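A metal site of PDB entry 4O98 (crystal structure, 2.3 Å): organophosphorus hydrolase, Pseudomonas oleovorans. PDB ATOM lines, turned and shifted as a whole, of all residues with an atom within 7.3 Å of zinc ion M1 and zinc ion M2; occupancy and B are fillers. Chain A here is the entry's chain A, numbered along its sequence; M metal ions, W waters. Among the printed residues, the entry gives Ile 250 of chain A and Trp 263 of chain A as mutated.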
ATOM      1  N   ALA A  88     -22.931 -25.034  -1.999  1.00  0.00           N
ATOM      2  CA  ALA A  88     -21.883 -26.060  -1.903  1.00  0.00           C
ATOM      3  C   ALA A  88     -20.797 -25.659  -0.904  1.00  0.00           C
ATOM      4  O   ALA A  88     -20.575 -24.469  -0.651  1.00  0.00           O
ATOM      5  CB  ALA A  88     -21.248 -26.336  -3.277  1.00  0.00           C
ATOM      6  N   VAL A  89     -20.143 -26.669  -0.316  1.00  0.00           N
ATOM      7  CA  VAL A  89     -18.967 -26.491   0.521  1.00  0.00           C
ATOM      8  C   VAL A  89     -17.878 -27.369  -0.088  1.00  0.00           C
ATOM      9  O   VAL A  89     -18.068 -28.583  -0.211  1.00  0.00           O
ATOM     10  CB  VAL A  89     -19.239 -26.905   1.968  1.00  0.00           C
ATOM     11  CG1 VAL A  89     -17.957 -26.810   2.811  1.00  0.00           C
ATOM     12  CG2 VAL A  89     -20.342 -26.045   2.581  1.00  0.00           C
ATOM     13  N   ASP A 104      -8.455 -26.456   3.154  1.00  0.00           N
ATOM     14  CA  ASP A 104      -9.756 -26.595   3.835  1.00  0.00           C
ATOM     15  C   ASP A 104     -10.194 -28.056   3.896  1.00  0.00           C
ATOM     16  O   ASP A 104      -9.590 -28.935   3.246  1.00  0.00           O
ATOM     17  CB  ASP A 104     -10.844 -25.683   3.243  1.00  0.00           C
ATOM     18  CG  ASP A 104     -10.518 -24.199   3.410  1.00  0.00           C
ATOM     19  OD1 ASP A 104      -9.755 -23.842   4.322  1.00  0.00           O
ATOM     20  OD2 ASP A 104     -11.038 -23.378   2.629  1.00  0.00           O
ATOM     21  N   PHE A 111     -22.128 -28.890  11.076  1.00  0.00           N
ATOM     22  CA  PHE A 111     -23.260 -28.191  10.468  1.00  0.00           C
ATOM     23  C   PHE A 111     -24.365 -29.157  10.040  1.00  0.00           C
ATOM     24  O   PHE A 111     -25.140 -28.856   9.135  1.00  0.00           O
ATOM     25  CB  PHE A 111     -22.827 -27.350   9.260  1.00  0.00           C
ATOM     26  CG  PHE A 111     -22.251 -26.003   9.620  1.00  0.00           C
ATOM     27  CD1 PHE A 111     -22.209 -25.579  10.932  1.00  0.00           C
ATOM     28  CD2 PHE A 111     -21.782 -25.152   8.640  1.00  0.00           C
ATOM     29  CE1 PHE A 111     -21.691 -24.329  11.271  1.00  0.00           C
ATOM     30  CE2 PHE A 111     -21.271 -23.902   8.957  1.00  0.00           C
ATOM     31  CZ  PHE A 111     -21.225 -23.491  10.273  1.00  0.00           C
ATOM     32  N   THR A 138      -8.011 -21.596   4.881  1.00  0.00           N
ATOM     33  CA  THR A 138      -8.287 -20.231   4.436  1.00  0.00           C
ATOM     34  C   THR A 138      -8.737 -19.392   5.628  1.00  0.00           C
ATOM     35  O   THR A 138      -8.396 -18.206   5.716  1.00  0.00           O
ATOM     36  CB  THR A 138      -9.331 -20.161   3.287  1.00  0.00           C
ATOM     37  OG1 THR A 138     -10.514 -20.895   3.661  1.00  0.00           O
ATOM     38  CG2 THR A 138      -8.751 -20.755   2.003  1.00  0.00           C
ATOM     39  N   HIS A 139      -9.488 -20.024   6.529  1.00  0.00           N
ATOM     40  CA  HIS A 139      -9.979 -19.403   7.769  1.00  0.00           C
ATOM     41  C   HIS A 139     -10.608 -20.485   8.650  1.00  0.00           C
ATOM     42  O   HIS A 139     -10.785 -21.630   8.208  1.00  0.00           O
ATOM     43  CB  HIS A 139     -10.986 -18.273   7.484  1.00  0.00           C
ATOM     44  CG  HIS A 139     -12.224 -18.699   6.748  1.00  0.00           C
ATOM     45  ND1 HIS A 139     -12.180 -19.346   5.531  1.00  0.00           N
ATOM     46  CD2 HIS A 139     -13.533 -18.541   7.046  1.00  0.00           C
ATOM     47  CE1 HIS A 139     -13.416 -19.573   5.112  1.00  0.00           C
ATOM     48  NE2 HIS A 139     -14.259 -19.102   6.011  1.00  0.00           N
ATOM     49  N   LEU A 140     -10.943 -20.130   9.895  1.00  0.00           N
ATOM     50  CA  LEU A 140     -11.323 -21.129  10.909  1.00  0.00           C
ATOM     51  C   LEU A 140     -12.826 -21.358  11.099  1.00  0.00           C
ATOM     52  O   LEU A 140     -13.243 -21.939  12.103  1.00  0.00           O
ATOM     53  CB  LEU A 140     -10.674 -20.819  12.273  1.00  0.00           C
ATOM     54  CG  LEU A 140      -9.200 -21.171  12.439  1.00  0.00           C
ATOM     55  CD1 LEU A 140      -8.656 -20.524  13.695  1.00  0.00           C
ATOM     56  CD2 LEU A 140      -9.002 -22.682  12.477  1.00  0.00           C
ATOM     57  N   HIS A 141     -13.641 -20.891  10.146  1.00  0.00           N
ATOM     58  CA  HIS A 141     -15.071 -21.197  10.169  1.00  0.00           C
ATOM     59  C   HIS A 141     -15.292 -22.711  10.176  1.00  0.00           C
ATOM     60  O   HIS A 141     -14.452 -23.459   9.658  1.00  0.00           O
ATOM     61  CB  HIS A 141     -15.764 -20.551   8.967  1.00  0.00           C
ATOM     62  CG  HIS A 141     -16.287 -19.173   9.251  1.00  0.00           C
ATOM     63  ND1 HIS A 141     -16.650 -18.301   8.242  1.00  0.00           N
ATOM     64  CD2 HIS A 141     -16.505 -18.526  10.416  1.00  0.00           C
ATOM     65  CE1 HIS A 141     -17.069 -17.165   8.783  1.00  0.00           C
ATOM     66  NE2 HIS A 141     -16.994 -17.277  10.098  1.00  0.00           N
ATOM     67  N   PRO A 142     -16.420 -23.159  10.767  1.00  0.00           N
ATOM     68  CA  PRO A 142     -16.648 -24.595  10.935  1.00  0.00           C
ATOM     69  C   PRO A 142     -16.650 -25.364   9.623  1.00  0.00           C
ATOM     70  O   PRO A 142     -16.187 -26.510   9.619  1.00  0.00           O
ATOM     71  CB  PRO A 142     -18.044 -24.652  11.564  1.00  0.00           C
ATOM     72  CG  PRO A 142     -18.192 -23.337  12.270  1.00  0.00           C
ATOM     73  CD  PRO A 142     -17.494 -22.357  11.363  1.00  0.00           C
ATOM     74  N   ASP A 143     -17.151 -24.754   8.542  1.00  0.00           N
ATOM     75  CA  ASP A 143     -17.269 -25.449   7.260  1.00  0.00           C
ATOM     76  C   ASP A 143     -15.936 -25.560   6.518  1.00  0.00           C
ATOM     77  O   ASP A 143     -15.887 -26.089   5.397  1.00  0.00           O
ATOM     78  CB  ASP A 143     -18.341 -24.825   6.340  1.00  0.00           C
ATOM     79  CG  ASP A 143     -18.170 -23.314   6.176  1.00  0.00           C
ATOM     80  OD1 ASP A 143     -17.939 -22.628   7.197  1.00  0.00           O
ATOM     81  OD2 ASP A 143     -18.295 -22.815   5.027  1.00  0.00           O
ATOM     82  N   HIS A 144     -14.868 -25.084   7.164  1.00  0.00           N
ATOM     83  CA  HIS A 144     -13.511 -25.185   6.606  1.00  0.00           C
ATOM     84  C   HIS A 144     -12.578 -25.956   7.542  1.00  0.00           C
ATOM     85  O   HIS A 144     -11.708 -26.703   7.081  1.00  0.00           O
ATOM     86  CB  HIS A 144     -12.961 -23.793   6.312  1.00  0.00           C
ATOM     87  CG  HIS A 144     -13.761 -23.053   5.290  1.00  0.00           C
ATOM     88  ND1 HIS A 144     -14.956 -22.439   5.589  1.00  0.00           N
ATOM     89  CD2 HIS A 144     -13.577 -22.905   3.956  1.00  0.00           C
ATOM     90  CE1 HIS A 144     -15.459 -21.910   4.494  1.00  0.00           C
ATOM     91  NE2 HIS A 144     -14.644 -22.175   3.483  1.00  0.00           N
ATOM     92  N   HIS A 226     -13.827 -11.302   5.663  1.00  0.00           N
ATOM     93  CA  HIS A 226     -14.826 -12.325   5.930  1.00  0.00           C
ATOM     94  C   HIS A 226     -14.559 -12.896   7.312  1.00  0.00           C
ATOM     95  O   HIS A 226     -15.504 -13.085   8.090  1.00  0.00           O
ATOM     96  CB  HIS A 226     -14.795 -13.402   4.850  1.00  0.00           C
ATOM     97  CG  HIS A 226     -15.685 -14.577   5.141  1.00  0.00           C
ATOM     98  ND1 HIS A 226     -17.060 -14.501   5.034  1.00  0.00           N
ATOM     99  CD2 HIS A 226     -15.398 -15.830   5.541  1.00  0.00           C
ATOM    100  CE1 HIS A 226     -17.581 -15.671   5.362  1.00  0.00           C
ATOM    101  NE2 HIS A 226     -16.590 -16.502   5.675  1.00  0.00           N
ATOM    102  N   THR A 227     -13.292 -13.162   7.613  1.00  0.00           N
ATOM    103  CA  THR A 227     -12.825 -13.304   9.004  1.00  0.00           C
ATOM    104  C   THR A 227     -11.553 -12.452   9.146  1.00  0.00           C
ATOM    105  O   THR A 227     -10.983 -12.017   8.120  1.00  0.00           O
ATOM    106  CB  THR A 227     -12.499 -14.764   9.383  1.00  0.00           C
ATOM    107  OG1 THR A 227     -11.393 -15.208   8.594  1.00  0.00           O
ATOM    108  CG2 THR A 227     -13.692 -15.684   9.158  1.00  0.00           C
ATOM    109  N   HIS A 230      -8.662 -14.171   7.217  1.00  0.00           N
ATOM    110  CA  HIS A 230      -9.030 -14.933   6.026  1.00  0.00           C
ATOM    111  C   HIS A 230      -7.939 -14.807   4.978  1.00  0.00           C
ATOM    112  O   HIS A 230      -7.473 -13.698   4.675  1.00  0.00           O
ATOM    113  CB  HIS A 230     -10.359 -14.431   5.455  1.00  0.00           C
ATOM    114  CG  HIS A 230     -10.861 -15.243   4.298  1.00  0.00           C
ATOM    115  ND1 HIS A 230     -10.495 -14.993   2.991  1.00  0.00           N
ATOM    116  CD2 HIS A 230     -11.672 -16.332   4.269  1.00  0.00           C
ATOM    117  CE1 HIS A 230     -11.077 -15.874   2.197  1.00  0.00           C
ATOM    118  NE2 HIS A 230     -11.801 -16.699   2.949  1.00  0.00           N
ATOM    119  N   GLY A 246     -10.987 -19.437  -0.867  1.00  0.00           N
ATOM    120  CA  GLY A 246     -11.810 -19.484   0.341  1.00  0.00           C
ATOM    121  C   GLY A 246     -13.175 -18.837   0.149  1.00  0.00           C
ATOM    122  O   GLY A 246     -13.906 -19.157  -0.799  1.00  0.00           O
ATOM    123  N   ASP A 247     -13.530 -17.940   1.062  1.00  0.00           N
ATOM    124  CA  ASP A 247     -14.863 -17.373   1.103  1.00  0.00           C
ATOM    125  C   ASP A 247     -14.904 -15.907   0.651  1.00  0.00           C
ATOM    126  O   ASP A 247     -15.602 -15.083   1.221  1.00  0.00           O
ATOM    127  CB  ASP A 247     -15.455 -17.516   2.509  1.00  0.00           C
ATOM    128  CG  ASP A 247     -15.951 -18.933   2.792  1.00  0.00           C
ATOM    129  OD1 ASP A 247     -15.517 -19.869   2.075  1.00  0.00           O
ATOM    130  OD2 ASP A 247     -16.765 -19.113   3.722  1.00  0.00           O
ATOM    131  N   LEU A 249     -16.460 -14.950  -1.608  1.00  0.00           N
ATOM    132  CA  LEU A 249     -17.776 -14.798  -2.169  1.00  0.00           C
ATOM    133  C   LEU A 249     -18.594 -16.015  -1.741  1.00  0.00           C
ATOM    134  O   LEU A 249     -18.058 -17.120  -1.697  1.00  0.00           O
ATOM    135  CB  LEU A 249     -17.592 -14.766  -3.681  1.00  0.00           C
ATOM    136  CG  LEU A 249     -18.696 -14.576  -4.691  1.00  0.00           C
ATOM    137  CD1 LEU A 249     -18.036 -13.978  -5.938  1.00  0.00           C
ATOM    138  CD2 LEU A 249     -19.325 -15.922  -4.965  1.00  0.00           C
ATOM    139  N   ILE A 250     -19.862 -15.809  -1.390  1.00  0.00           N
ATOM    140  CA  ILE A 250     -20.684 -16.921  -0.904  1.00  0.00           C
ATOM    141  C   ILE A 250     -21.782 -17.344  -1.886  1.00  0.00           C
ATOM    142  O   ILE A 250     -22.182 -18.509  -1.919  1.00  0.00           O
ATOM    143  CB  ILE A 250     -21.321 -16.615   0.470  1.00  0.00           C
ATOM    144  CG1 ILE A 250     -20.311 -16.001   1.437  1.00  0.00           C
ATOM    145  CG2 ILE A 250     -21.940 -17.896   1.078  1.00  0.00           C
ATOM    146  CD1 ILE A 250     -19.358 -17.028   2.105  1.00  0.00           C
ATOM    147  N   TRP A 263     -22.332 -10.381   3.027  1.00  0.00           N
ATOM    148  CA  TRP A 263     -22.898 -11.550   3.689  1.00  0.00           C
ATOM    149  C   TRP A 263     -22.991 -11.280   5.185  1.00  0.00           C
ATOM    150  O   TRP A 263     -22.031 -10.761   5.793  1.00  0.00           O
ATOM    151  CB  TRP A 263     -21.966 -12.735   3.422  1.00  0.00           C
ATOM    152  CG  TRP A 263     -22.456 -14.031   3.927  1.00  0.00           C
ATOM    153  CD1 TRP A 263     -21.924 -14.777   4.948  1.00  0.00           C
ATOM    154  CD2 TRP A 263     -23.559 -14.767   3.421  1.00  0.00           C
ATOM    155  NE1 TRP A 263     -22.641 -15.933   5.105  1.00  0.00           N
ATOM    156  CE2 TRP A 263     -23.654 -15.944   4.189  1.00  0.00           C
ATOM    157  CE3 TRP A 263     -24.486 -14.548   2.397  1.00  0.00           C
ATOM    158  CZ2 TRP A 263     -24.638 -16.909   3.949  1.00  0.00           C
ATOM    159  CZ3 TRP A 263     -25.452 -15.492   2.161  1.00  0.00           C
ATOM    160  CH2 TRP A 263     -25.525 -16.660   2.937  1.00  0.00           C
ATOM    161  N   PHE A 265     -22.648 -13.023   7.769  1.00  0.00           N
ATOM    162  CA  PHE A 265     -21.612 -13.601   8.616  1.00  0.00           C
ATOM    163  C   PHE A 265     -20.166 -13.258   8.234  1.00  0.00           C
ATOM    164  O   PHE A 265     -19.234 -13.911   8.710  1.00  0.00           O
ATOM    165  CB  PHE A 265     -21.779 -15.111   8.751  1.00  0.00           C
ATOM    166  CG  PHE A 265     -23.041 -15.502   9.443  1.00  0.00           C
ATOM    167  CD1 PHE A 265     -24.228 -15.657   8.730  1.00  0.00           C
ATOM    168  CD2 PHE A 265     -23.064 -15.692  10.818  1.00  0.00           C
ATOM    169  CE1 PHE A 265     -25.413 -16.001   9.376  1.00  0.00           C
ATOM    170  CE2 PHE A 265     -24.237 -16.038  11.470  1.00  0.00           C
ATOM    171  CZ  PHE A 265     -25.419 -16.187  10.751  1.00  0.00           C
ATOM    172  N   ASP A 266     -19.993 -12.261   7.368  1.00  0.00           N
ATOM    173  CA  ASP A 266     -18.686 -11.617   7.261  1.00  0.00           C
ATOM    174  C   ASP A 266     -18.426 -10.894   8.590  1.00  0.00           C
ATOM    175  O   ASP A 266     -19.204 -10.024   8.988  1.00  0.00           O
ATOM    176  CB  ASP A 266     -18.672 -10.575   6.134  1.00  0.00           C
ATOM    177  CG  ASP A 266     -18.702 -11.200   4.738  1.00  0.00           C
ATOM    178  OD1 ASP A 266     -18.093 -12.274   4.543  1.00  0.00           O
ATOM    179  OD2 ASP A 266     -19.318 -10.583   3.830  1.00  0.00           O
ATOM    180  N   ALA A 293     -14.596 -22.104  -2.432  1.00  0.00           N
ATOM    181  CA  ALA A 293     -15.198 -23.019  -1.464  1.00  0.00           C
ATOM    182  C   ALA A 293     -16.724 -23.108  -1.552  1.00  0.00           C
ATOM    183  O   ALA A 293     -17.306 -24.142  -1.219  1.00  0.00           O
ATOM    184  CB  ALA A 293     -14.779 -22.633  -0.062  1.00  0.00           C
ATOM    185  N   HIS A 294     -17.381 -22.036  -1.961  1.00  0.00           N
ATOM    186  CA  HIS A 294     -18.837 -22.034  -2.008  1.00  0.00           C
ATOM    187  C   HIS A 294     -19.357 -21.785  -3.425  1.00  0.00           C
ATOM    188  O   HIS A 294     -20.535 -21.448  -3.612  1.00  0.00           O
ATOM    189  CB  HIS A 294     -19.405 -21.011  -1.000  1.00  0.00           C
ATOM    190  CG  HIS A 294     -19.025 -21.290   0.421  1.00  0.00           C
ATOM    191  ND1 HIS A 294     -19.337 -22.489   1.046  1.00  0.00           N
ATOM    192  CD2 HIS A 294     -18.343 -20.555   1.329  1.00  0.00           C
ATOM    193  CE1 HIS A 294     -18.871 -22.460   2.285  1.00  0.00           C
ATOM    194  NE2 HIS A 294     -18.270 -21.301   2.483  1.00  0.00           N
HETATM  195 ZN    ZN M   1     -16.516 -18.640   6.050  1.00  0.00          ZN
HETATM  196 ZN    ZN M   2     -17.290 -21.049   4.192  1.00  0.00          ZN
HETATM  197  O   HOH W   1     -17.971 -20.167   6.178  1.00  0.00           O
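His 144 touches zinc ion M1. The nearest printed residue that does not touch zinc ion M1 is Asp 143 (4.4 Å).
Zinc ion M2 is bound by NE2 of His 294 (2.0 Å), OD2 of Asp 247 (2.1 Å), OD2 of Asp 143 (2.2 Å) and water W1 (2.3 Å). Zinc ion M2 has four donor atoms within binding distance.
His 144 touches zinc ion M2. Of the 23 residues printed, 4 come within 4 Å of zinc ion M2.
Zinc ion M1 is bound by water W1 (2.1 Å), a ring nitrogen (NE2) of His 226 (2.2 Å), a ring nitrogen (ND1) of His 141 (2.2 Å), a ring nitrogen (NE2) of His 139 (2.3 Å) and the side-chain carboxylate of Asp 247 (2.4 Å). Zinc ion M1 has five donor atoms within binding distance.
N of Asp 247 is in hydrogen-bond range of NE2 of His 230. A ring nitrogen (ND1) of His 144 sits close to the side-chain carboxylate of Asp 143 (3.4 Å). A ring nitrogen (ND1) of His 226 is in hydrogen-bond range of the side-chain carboxylate (OD1) of Asp 266 (2.5 Å). A ring nitrogen (ND1) of His 294 lies within hydrogen-bond range of the backbone carbonyl oxygen (O) of Ala 88, at 2.9 Å. A ring nitrogen (ND1) of His 139 is in hydrogen-bond range of the side-chain hydroxyl (OG1) of Thr 138 (2.9 Å). A ring nitrogen (NE2) of His 144 lies within hydrogen-bond range of the side-chain carboxylate (OD1) of Asp 247 (2.8 Å). NE2 of His 139 sits close to ND1 of His 144 (3.4 Å).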
